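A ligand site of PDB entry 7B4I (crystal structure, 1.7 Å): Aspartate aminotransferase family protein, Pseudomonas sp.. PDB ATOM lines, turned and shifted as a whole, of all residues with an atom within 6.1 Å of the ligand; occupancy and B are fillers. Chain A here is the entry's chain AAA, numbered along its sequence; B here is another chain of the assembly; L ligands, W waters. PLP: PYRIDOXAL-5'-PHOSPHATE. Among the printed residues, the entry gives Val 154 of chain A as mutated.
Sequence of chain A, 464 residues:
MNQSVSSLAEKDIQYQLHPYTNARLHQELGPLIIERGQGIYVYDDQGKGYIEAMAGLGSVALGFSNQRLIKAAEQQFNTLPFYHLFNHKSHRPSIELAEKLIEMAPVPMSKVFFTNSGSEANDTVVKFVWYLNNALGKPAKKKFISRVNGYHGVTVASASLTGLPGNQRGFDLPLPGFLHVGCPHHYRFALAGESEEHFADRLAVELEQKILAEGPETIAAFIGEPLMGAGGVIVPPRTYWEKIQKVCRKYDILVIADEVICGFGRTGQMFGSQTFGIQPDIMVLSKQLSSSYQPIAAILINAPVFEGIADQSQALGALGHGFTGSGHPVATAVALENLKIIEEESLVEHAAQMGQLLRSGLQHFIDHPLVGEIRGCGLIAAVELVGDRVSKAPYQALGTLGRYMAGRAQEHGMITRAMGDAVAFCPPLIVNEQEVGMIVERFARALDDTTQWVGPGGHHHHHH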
ATOM      1  N   LEU A  57      -9.363  19.654 -29.650  1.00  0.00           N
ATOM      2  CA  LEU A  57      -8.612  18.425 -30.015  1.00  0.00           C
ATOM      3  C   LEU A  57      -9.633  17.330 -30.317  1.00  0.00           C
ATOM      4  O   LEU A  57      -9.546  16.258 -29.722  1.00  0.00           O
ATOM      5  CB  LEU A  57      -7.642  18.079 -28.885  1.00  0.00           C
ATOM      6  CG  LEU A  57      -6.550  19.128 -28.639  1.00  0.00           C
ATOM      7  CD1 LEU A  57      -5.732  18.792 -27.401  1.00  0.00           C
ATOM      8  CD2 LEU A  57      -5.660  19.270 -29.871  1.00  0.00           C
ATOM      9  N   ASN A 116      -8.471  10.238 -15.634  1.00  0.00           N
ATOM     10  CA  ASN A 116      -8.525  11.654 -16.084  1.00  0.00           C
ATOM     11  C   ASN A 116      -8.369  11.744 -17.589  1.00  0.00           C
ATOM     12  O   ASN A 116      -8.982  12.606 -18.174  1.00  0.00           O
ATOM     13  CB  ASN A 116      -7.446  12.487 -15.397  1.00  0.00           C
ATOM     14  CG  ASN A 116      -7.491  12.344 -13.907  1.00  0.00           C
ATOM     15  OD1 ASN A 116      -8.443  12.801 -13.291  1.00  0.00           O
ATOM     16  ND2 ASN A 116      -6.476  11.687 -13.351  1.00  0.00           N
ATOM     17  N   SER A 117      -7.544  10.908 -18.209  1.00  0.00           N
ATOM     18  CA  SER A 117      -7.143  11.083 -19.619  1.00  0.00           C
ATOM     19  C   SER A 117      -7.274   9.763 -20.391  1.00  0.00           C
ATOM     20  O   SER A 117      -7.221   8.702 -19.754  1.00  0.00           O
ATOM     21  CB  SER A 117      -5.728  11.590 -19.727  1.00  0.00           C
ATOM     22  OG  SER A 117      -4.804  10.612 -19.283  1.00  0.00           O
ATOM     23  N   GLY A 118      -7.368   9.884 -21.712  1.00  0.00           N
ATOM     24  CA  GLY A 118      -7.273   8.734 -22.633  1.00  0.00           C
ATOM     25  C   GLY A 118      -5.951   8.008 -22.460  1.00  0.00           C
ATOM     26  O   GLY A 118      -5.945   6.755 -22.477  1.00  0.00           O
ATOM     27  N   SER A 119      -4.846   8.731 -22.280  1.00  0.00           N
ATOM     28  CA  SER A 119      -3.504   8.125 -22.064  1.00  0.00           C
ATOM     29  C   SER A 119      -3.538   7.252 -20.806  1.00  0.00           C
ATOM     30  O   SER A 119      -3.077   6.106 -20.871  1.00  0.00           O
ATOM     31  CB  SER A 119      -2.414   9.158 -21.974  1.00  0.00           C
ATOM     32  OG  SER A 119      -2.292   9.904 -23.175  1.00  0.00           O
ATOM     33  N   GLU A 120      -4.008   7.798 -19.670  1.00  0.00           N
ATOM     34  CA  GLU A 120      -4.138   7.023 -18.413  1.00  0.00           C
ATOM     35  C   GLU A 120      -5.055   5.811 -18.644  1.00  0.00           C
ATOM     36  O   GLU A 120      -4.758   4.735 -18.059  1.00  0.00           O
ATOM     37  CB  GLU A 120      -4.796   7.825 -17.304  1.00  0.00           C
ATOM     38  CG  GLU A 120      -3.886   8.835 -16.633  1.00  0.00           C
ATOM     39  CD  GLU A 120      -4.714   9.761 -15.749  1.00  0.00           C
ATOM     40  OE1 GLU A 120      -5.954   9.732 -15.920  1.00  0.00           O
ATOM     41  OE2 GLU A 120      -4.155  10.496 -14.906  1.00  0.00           O
ATOM     42  N   ASN A 122      -5.743   4.042 -21.443  1.00  0.00           N
ATOM     43  CA  ASN A 122      -5.085   2.961 -22.231  1.00  0.00           C
ATOM     44  C   ASN A 122      -3.963   2.336 -21.403  1.00  0.00           C
ATOM     45  O   ASN A 122      -3.756   1.107 -21.513  1.00  0.00           O
ATOM     46  CB  ASN A 122      -4.611   3.443 -23.593  1.00  0.00           C
ATOM     47  CG  ASN A 122      -5.758   3.549 -24.569  1.00  0.00           C
ATOM     48  OD1 ASN A 122      -6.711   2.753 -24.550  1.00  0.00           O
ATOM     49  ND2 ASN A 122      -5.700   4.553 -25.419  1.00  0.00           N
ATOM     50  N   TYR A 151      -3.118   6.171 -32.656  1.00  0.00           N
ATOM     51  CA  TYR A 151      -2.864   7.076 -31.503  1.00  0.00           C
ATOM     52  C   TYR A 151      -3.640   6.560 -30.291  1.00  0.00           C
ATOM     53  O   TYR A 151      -4.872   6.468 -30.352  1.00  0.00           O
ATOM     54  CB  TYR A 151      -3.237   8.519 -31.805  1.00  0.00           C
ATOM     55  CG  TYR A 151      -2.758   9.475 -30.755  1.00  0.00           C
ATOM     56  CD1 TYR A 151      -1.414   9.785 -30.660  1.00  0.00           C
ATOM     57  CD2 TYR A 151      -3.622  10.091 -29.867  1.00  0.00           C
ATOM     58  CE1 TYR A 151      -0.932  10.696 -29.726  1.00  0.00           C
ATOM     59  CE2 TYR A 151      -3.150  10.993 -28.913  1.00  0.00           C
ATOM     60  CZ  TYR A 151      -1.812  11.302 -28.850  1.00  0.00           C
ATOM     61  OH  TYR A 151      -1.290  12.214 -27.959  1.00  0.00           O
ATOM     62  N   HIS A 152      -2.912   6.271 -29.231  1.00  0.00           N
ATOM     63  CA  HIS A 152      -3.461   5.695 -27.982  1.00  0.00           C
ATOM     64  C   HIS A 152      -2.947   6.479 -26.772  1.00  0.00           C
ATOM     65  O   HIS A 152      -3.177   6.025 -25.650  1.00  0.00           O
ATOM     66  CB  HIS A 152      -3.161   4.188 -27.948  1.00  0.00           C
ATOM     67  CG  HIS A 152      -3.745   3.479 -29.117  1.00  0.00           C
ATOM     68  ND1 HIS A 152      -5.108   3.386 -29.316  1.00  0.00           N
ATOM     69  CD2 HIS A 152      -3.152   2.898 -30.184  1.00  0.00           C
ATOM     70  CE1 HIS A 152      -5.336   2.759 -30.458  1.00  0.00           C
ATOM     71  NE2 HIS A 152      -4.158   2.441 -30.996  1.00  0.00           N
ATOM     72  N   GLY A 153      -2.274   7.602 -26.982  1.00  0.00           N
ATOM     73  CA  GLY A 153      -1.822   8.480 -25.901  1.00  0.00           C
ATOM     74  C   GLY A 153      -0.312   8.464 -25.728  1.00  0.00           C
ATOM     75  O   GLY A 153       0.378   7.927 -26.622  1.00  0.00           O
ATOM     76  N   VAL A 154       0.161   9.008 -24.602  1.00  0.00           N
ATOM     77  CA  VAL A 154       1.553   9.509 -24.483  1.00  0.00           C
ATOM     78  C   VAL A 154       2.241   9.001 -23.219  1.00  0.00           C
ATOM     79  O   VAL A 154       3.379   9.417 -22.997  1.00  0.00           O
ATOM     80  CB  VAL A 154       1.610  11.044 -24.563  1.00  0.00           C
ATOM     81  CG1 VAL A 154       1.095  11.528 -25.895  1.00  0.00           C
ATOM     82  CG2 VAL A 154       0.868  11.715 -23.415  1.00  0.00           C
ATOM     83  N   GLU A 225      -8.319   2.247 -32.804  1.00  0.00           N
ATOM     84  CA  GLU A 225      -9.377   3.236 -33.051  1.00  0.00           C
ATOM     85  C   GLU A 225     -10.227   2.719 -34.212  1.00  0.00           C
ATOM     86  O   GLU A 225      -9.660   2.283 -35.210  1.00  0.00           O
ATOM     87  CB  GLU A 225      -8.752   4.562 -33.484  1.00  0.00           C
ATOM     88  CG  GLU A 225      -7.817   5.196 -32.475  1.00  0.00           C
ATOM     89  CD  GLU A 225      -6.862   6.148 -33.189  1.00  0.00           C
ATOM     90  OE1 GLU A 225      -7.207   7.336 -33.346  1.00  0.00           O
ATOM     91  OE2 GLU A 225      -5.800   5.669 -33.679  1.00  0.00           O
ATOM     92  N   GLY A 229      -7.877   8.738 -35.888  1.00  0.00           N
ATOM     93  CA  GLY A 229      -8.073  10.198 -35.835  1.00  0.00           C
ATOM     94  C   GLY A 229      -6.766  10.948 -36.031  1.00  0.00           C
ATOM     95  O   GLY A 229      -6.538  11.475 -37.128  1.00  0.00           O
ATOM     96  N   ALA A 230      -5.924  11.003 -34.996  1.00  0.00           N
ATOM     97  CA  ALA A 230      -4.657  11.768 -34.985  1.00  0.00           C
ATOM     98  C   ALA A 230      -3.748  11.295 -36.113  1.00  0.00           C
ATOM     99  O   ALA A 230      -2.946  12.100 -36.581  1.00  0.00           O
ATOM    100  CB  ALA A 230      -3.992  11.631 -33.637  1.00  0.00           C
ATOM    101  N   ASP A 258     -10.519   1.691 -29.041  1.00  0.00           N
ATOM    102  CA  ASP A 258     -10.138   3.036 -28.528  1.00  0.00           C
ATOM    103  C   ASP A 258     -11.076   4.029 -29.200  1.00  0.00           C
ATOM    104  O   ASP A 258     -10.835   4.390 -30.352  1.00  0.00           O
ATOM    105  CB  ASP A 258      -8.652   3.318 -28.771  1.00  0.00           C
ATOM    106  CG  ASP A 258      -8.225   4.650 -28.171  1.00  0.00           C
ATOM    107  OD1 ASP A 258      -9.143   5.471 -27.896  1.00  0.00           O
ATOM    108  OD2 ASP A 258      -7.013   4.849 -27.990  1.00  0.00           O
ATOM    109  N   GLU A 259     -12.142   4.438 -28.496  1.00  0.00           N
ATOM    110  CA  GLU A 259     -13.194   5.351 -28.999  1.00  0.00           C
ATOM    111  C   GLU A 259     -12.934   6.775 -28.481  1.00  0.00           C
ATOM    112  O   GLU A 259     -13.892   7.550 -28.385  1.00  0.00           O
ATOM    113  CB  GLU A 259     -14.560   4.845 -28.512  1.00  0.00           C
ATOM    114  CG  GLU A 259     -14.956   3.527 -29.139  1.00  0.00           C
ATOM    115  CD  GLU A 259     -16.059   3.630 -30.177  1.00  0.00           C
ATOM    116  OE1 GLU A 259     -16.403   4.758 -30.605  1.00  0.00           O
ATOM    117  OE2 GLU A 259     -16.595   2.557 -30.554  1.00  0.00           O
ATOM    118  N   VAL A 260     -11.690   7.124 -28.134  1.00  0.00           N
ATOM    119  CA  VAL A 260     -11.428   8.467 -27.556  1.00  0.00           C
ATOM    120  C   VAL A 260     -11.879   9.566 -28.540  1.00  0.00           C
ATOM    121  O   VAL A 260     -12.484  10.560 -28.068  1.00  0.00           O
ATOM    122  CB  VAL A 260      -9.968   8.627 -27.106  1.00  0.00           C
ATOM    123  CG1 VAL A 260      -9.597  10.104 -26.876  1.00  0.00           C
ATOM    124  CG2 VAL A 260      -9.713   7.817 -25.842  1.00  0.00           C
ATOM    125  N   ILE A 261     -11.640   9.404 -29.845  1.00  0.00           N
ATOM    126  CA  ILE A 261     -12.159  10.383 -30.852  1.00  0.00           C
ATOM    127  C   ILE A 261     -13.545   9.965 -31.365  1.00  0.00           C
ATOM    128  O   ILE A 261     -14.410  10.857 -31.472  1.00  0.00           O
ATOM    129  CB  ILE A 261     -11.145  10.587 -31.992  1.00  0.00           C
ATOM    130  CG1 ILE A 261     -10.032  11.542 -31.565  1.00  0.00           C
ATOM    131  CG2 ILE A 261     -11.821  11.089 -33.252  1.00  0.00           C
ATOM    132  CD1 ILE A 261     -10.462  12.998 -31.537  1.00  0.00           C
ATOM    133  N   SER A 286     -13.167   9.155 -24.007  1.00  0.00           N
ATOM    134  CA  SER A 286     -12.710  10.449 -23.423  1.00  0.00           C
ATOM    135  C   SER A 286     -13.234  11.594 -24.277  1.00  0.00           C
ATOM    136  O   SER A 286     -14.234  11.395 -24.973  1.00  0.00           O
ATOM    137  CB  SER A 286     -11.194  10.482 -23.279  1.00  0.00           C
ATOM    138  OG  SER A 286     -10.821  11.553 -22.416  1.00  0.00           O
ATOM    139  N   LYS A 287     -12.571  12.749 -24.222  1.00  0.00           N
ATOM    140  CA  LYS A 287     -12.755  13.876 -25.179  1.00  0.00           C
ATOM    141  C   LYS A 287     -14.234  14.285 -25.186  1.00  0.00           C
ATOM    142  O   LYS A 287     -14.648  15.012 -24.253  1.00  0.00           O
ATOM    143  CB  LYS A 287     -12.159  13.537 -26.548  1.00  0.00           C
ATOM    144  CG  LYS A 287     -10.629  13.656 -26.577  1.00  0.00           C
ATOM    145  CD  LYS A 287      -9.990  13.531 -27.950  1.00  0.00           C
ATOM    146  CE  LYS A 287      -8.492  13.848 -27.945  1.00  0.00           C
ATOM    147  NZ  LYS A 287      -7.674  12.659 -28.292  1.00  0.00           N
ATOM    148  N   PHE B  86      -1.174  22.931 -27.341  1.00  0.00           N
ATOM    149  CA  PHE B  86      -0.399  22.252 -28.405  1.00  0.00           C
ATOM    150  C   PHE B  86      -0.009  23.279 -29.473  1.00  0.00           C
ATOM    151  O   PHE B  86      -0.780  24.225 -29.694  1.00  0.00           O
ATOM    152  CB  PHE B  86      -1.172  21.125 -29.081  1.00  0.00           C
ATOM    153  CG  PHE B  86      -1.529  19.903 -28.258  1.00  0.00           C
ATOM    154  CD1 PHE B  86      -1.459  19.893 -26.872  1.00  0.00           C
ATOM    155  CD2 PHE B  86      -2.000  18.767 -28.889  1.00  0.00           C
ATOM    156  CE1 PHE B  86      -1.846  18.776 -26.142  1.00  0.00           C
ATOM    157  CE2 PHE B  86      -2.363  17.647 -28.163  1.00  0.00           C
ATOM    158  CZ  PHE B  86      -2.269  17.640 -26.793  1.00  0.00           C
ATOM    159  N   ASN B 116      -2.693  16.130 -16.046  1.00  0.00           N
ATOM    160  CA  ASN B 116      -3.937  15.999 -15.229  1.00  0.00           C
ATOM    161  C   ASN B 116      -3.617  15.414 -13.850  1.00  0.00           C
ATOM    162  O   ASN B 116      -4.247  15.805 -12.889  1.00  0.00           O
ATOM    163  CB  ASN B 116      -4.968  15.111 -15.935  1.00  0.00           C
ATOM    164  CG  ASN B 116      -5.243  15.572 -17.340  1.00  0.00           C
ATOM    165  OD1 ASN B 116      -5.847  16.632 -17.534  1.00  0.00           O
ATOM    166  ND2 ASN B 116      -4.815  14.802 -18.323  1.00  0.00           N
ATOM    167  N   GLU B 120       0.552  10.756 -14.240  1.00  0.00           N
ATOM    168  CA  GLU B 120       0.953  11.275 -15.576  1.00  0.00           C
ATOM    169  C   GLU B 120       2.219  12.130 -15.447  1.00  0.00           C
ATOM    170  O   GLU B 120       3.087  12.078 -16.380  1.00  0.00           O
ATOM    171  CB  GLU B 120      -0.104  12.188 -16.185  1.00  0.00           C
ATOM    172  CG  GLU B 120      -1.281  11.485 -16.798  1.00  0.00           C
ATOM    173  CD  GLU B 120      -2.366  12.493 -17.130  1.00  0.00           C
ATOM    174  OE1 GLU B 120      -2.249  13.643 -16.651  1.00  0.00           O
ATOM    175  OE2 GLU B 120      -3.327  12.157 -17.851  1.00  0.00           O
ATOM    176  N   GLY B 322       2.171  15.266 -24.889  1.00  0.00           N
ATOM    177  CA  GLY B 322       1.172  16.176 -24.327  1.00  0.00           C
ATOM    178  C   GLY B 322      -0.122  15.457 -24.082  1.00  0.00           C
ATOM    179  O   GLY B 322      -0.410  14.530 -24.828  1.00  0.00           O
ATOM    180  N   PHE B 323      -0.903  15.918 -23.109  1.00  0.00           N
ATOM    181  CA  PHE B 323      -2.253  15.400 -22.826  1.00  0.00           C
ATOM    182  C   PHE B 323      -3.257  16.468 -23.277  1.00  0.00           C
ATOM    183  O   PHE B 323      -2.986  17.668 -23.149  1.00  0.00           O
ATOM    184  CB  PHE B 323      -2.388  15.134 -21.341  1.00  0.00           C
ATOM    185  CG  PHE B 323      -1.354  14.193 -20.795  1.00  0.00           C
ATOM    186  CD1 PHE B 323      -1.565  12.829 -20.809  1.00  0.00           C
ATOM    187  CD2 PHE B 323      -0.169  14.666 -20.258  1.00  0.00           C
ATOM    188  CE1 PHE B 323      -0.616  11.954 -20.308  1.00  0.00           C
ATOM    189  CE2 PHE B 323       0.787  13.798 -19.745  1.00  0.00           C
ATOM    190  CZ  PHE B 323       0.554  12.441 -19.778  1.00  0.00           C
ATOM    191  N   THR B 324      -4.393  16.029 -23.798  1.00  0.00           N
ATOM    192  CA  THR B 324      -5.529  16.908 -24.167  1.00  0.00           C
ATOM    193  C   THR B 324      -5.768  17.933 -23.045  1.00  0.00           C
ATOM    194  O   THR B 324      -5.857  19.139 -23.343  1.00  0.00           O
ATOM    195  CB  THR B 324      -6.787  16.083 -24.427  1.00  0.00           C
ATOM    196  OG1 THR B 324      -6.519  15.248 -25.540  1.00  0.00           O
ATOM    197  CG2 THR B 324      -8.011  16.939 -24.729  1.00  0.00           C
ATOM    198  N   GLY B 325      -5.804  17.466 -21.799  1.00  0.00           N
ATOM    199  CA  GLY B 325      -6.092  18.300 -20.627  1.00  0.00           C
ATOM    200  C   GLY B 325      -4.891  19.078 -20.088  1.00  0.00           C
ATOM    201  O   GLY B 325      -5.090  19.754 -19.071  1.00  0.00           O
HETATM  202  N1  PLP L   1      -6.658   7.680 -27.945  1.00  0.00           N
HETATM  203  C2  PLP L   1      -7.161   8.471 -28.971  1.00  0.00           C
HETATM  204  C2A PLP L   1      -7.858   7.828 -30.152  1.00  0.00           C
HETATM  205  C3  PLP L   1      -7.013   9.874 -28.938  1.00  0.00           C
HETATM  206  O3  PLP L   1      -7.518  10.635 -29.948  1.00  0.00           O
HETATM  207  C4  PLP L   1      -6.444  10.500 -27.806  1.00  0.00           C
HETATM  208  C4A PLP L   1      -6.773  11.958 -27.523  1.00  0.00           C
HETATM  209  C5  PLP L   1      -5.915   9.699 -26.772  1.00  0.00           C
HETATM  210  C6  PLP L   1      -6.024   8.290 -26.836  1.00  0.00           C
HETATM  211  C5A PLP L   1      -5.131  10.365 -25.586  1.00  0.00           C
HETATM  212  O4P PLP L   1      -6.002  11.175 -24.814  1.00  0.00           O
HETATM  213  P   PLP L   1      -5.388  12.261 -23.717  1.00  0.00           P
HETATM  214  O1P PLP L   1      -4.764  13.399 -24.478  1.00  0.00           O
HETATM  215  O2P PLP L   1      -6.520  12.788 -22.834  1.00  0.00           O
HETATM  216  O3P PLP L   1      -4.329  11.591 -22.853  1.00  0.00           O
HETATM  217  O   HOH W   1      -9.247  13.667 -22.888  1.00  0.00           O
HETATM  218  O   HOH W   2      -2.604  13.196 -25.934  1.00  0.00           O
HETATM  219  O   HOH W   3      -6.047  14.676 -21.068  1.00  0.00           O
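NZ of Lys 287 is covalently linked to C4A of the ligand. An oxygen (O3P) of the ligand lies close to the backbone NH (N) of Ser 119 (3.0 Å). OG of Ser 119 lies close to O3P of the ligand (2.7 Å). The backbone NH (N) of Thr 324 of chain B lies close to an oxygen (O1P) of the ligand (2.7 Å). OG1 of Thr 324 of chain B sits close to O1P of the ligand, at 2.8 Å. OD2 of Asp 258 lies close to N1 of the ligand, at 2.9 Å. The backbone NH (N) of Gly 118 lies close to an oxygen (O2P) of the ligand, at 3.2 Å. The backbone carbonyl oxygen (O) of Tyr 151 lies close to a nitrogen (N1) of the ligand (3.2 Å).
N of Val 154 is in hydrogen-bond range of OG of Ser 119 (3.0 Å). N of Val 260 lies within hydrogen-bond range of OD1 of Asp 258, at 3.0 Å. ND1 of His 152 is in hydrogen-bond range of OD2 of Asp 258 (2.7 Å). ND2 of Asn 122 sits at hydrogen-bond distance from OD2 of Asp 258 (2.9 Å). OE2 of Glu 225 sits at hydrogen-bond distance from N of Tyr 151 (2.9 Å). The backbone NH (N) of Gly 229 lies within hydrogen-bond range of the side-chain carboxylate (OE1) of Glu 225, at 3.0 Å. OG of Ser 117 sits at hydrogen-bond distance from OE2 of Glu 120 of chain B, at 2.6 Å. The backbone carbonyl oxygen of His 152 sits at hydrogen-bond distance from the side-chain amide nitrogen of Asn 122.
Merely in contact with the ligand: Ile 261 (3.1 Å), Glu 225 (3.3 Å), Val 260 (3.3 Å), Ser 117 (3.4 Å), His 152 (3.6 Å), Phe 323 of chain B (3.6 Å) and Gly 153 (3.8 Å). 13 residues have an atom within 4 Å of the ligand: Ser 117, Gly 118, Ser 119, Tyr 151, His 152, Gly 153, Glu 225, Asp 258, Val 260, Ile 261, Lys 287, Phe 323 of chain B and Thr 324 of chain B.
Water W2 bridges OH of Tyr 151 and O of Gly 322 of chain B.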
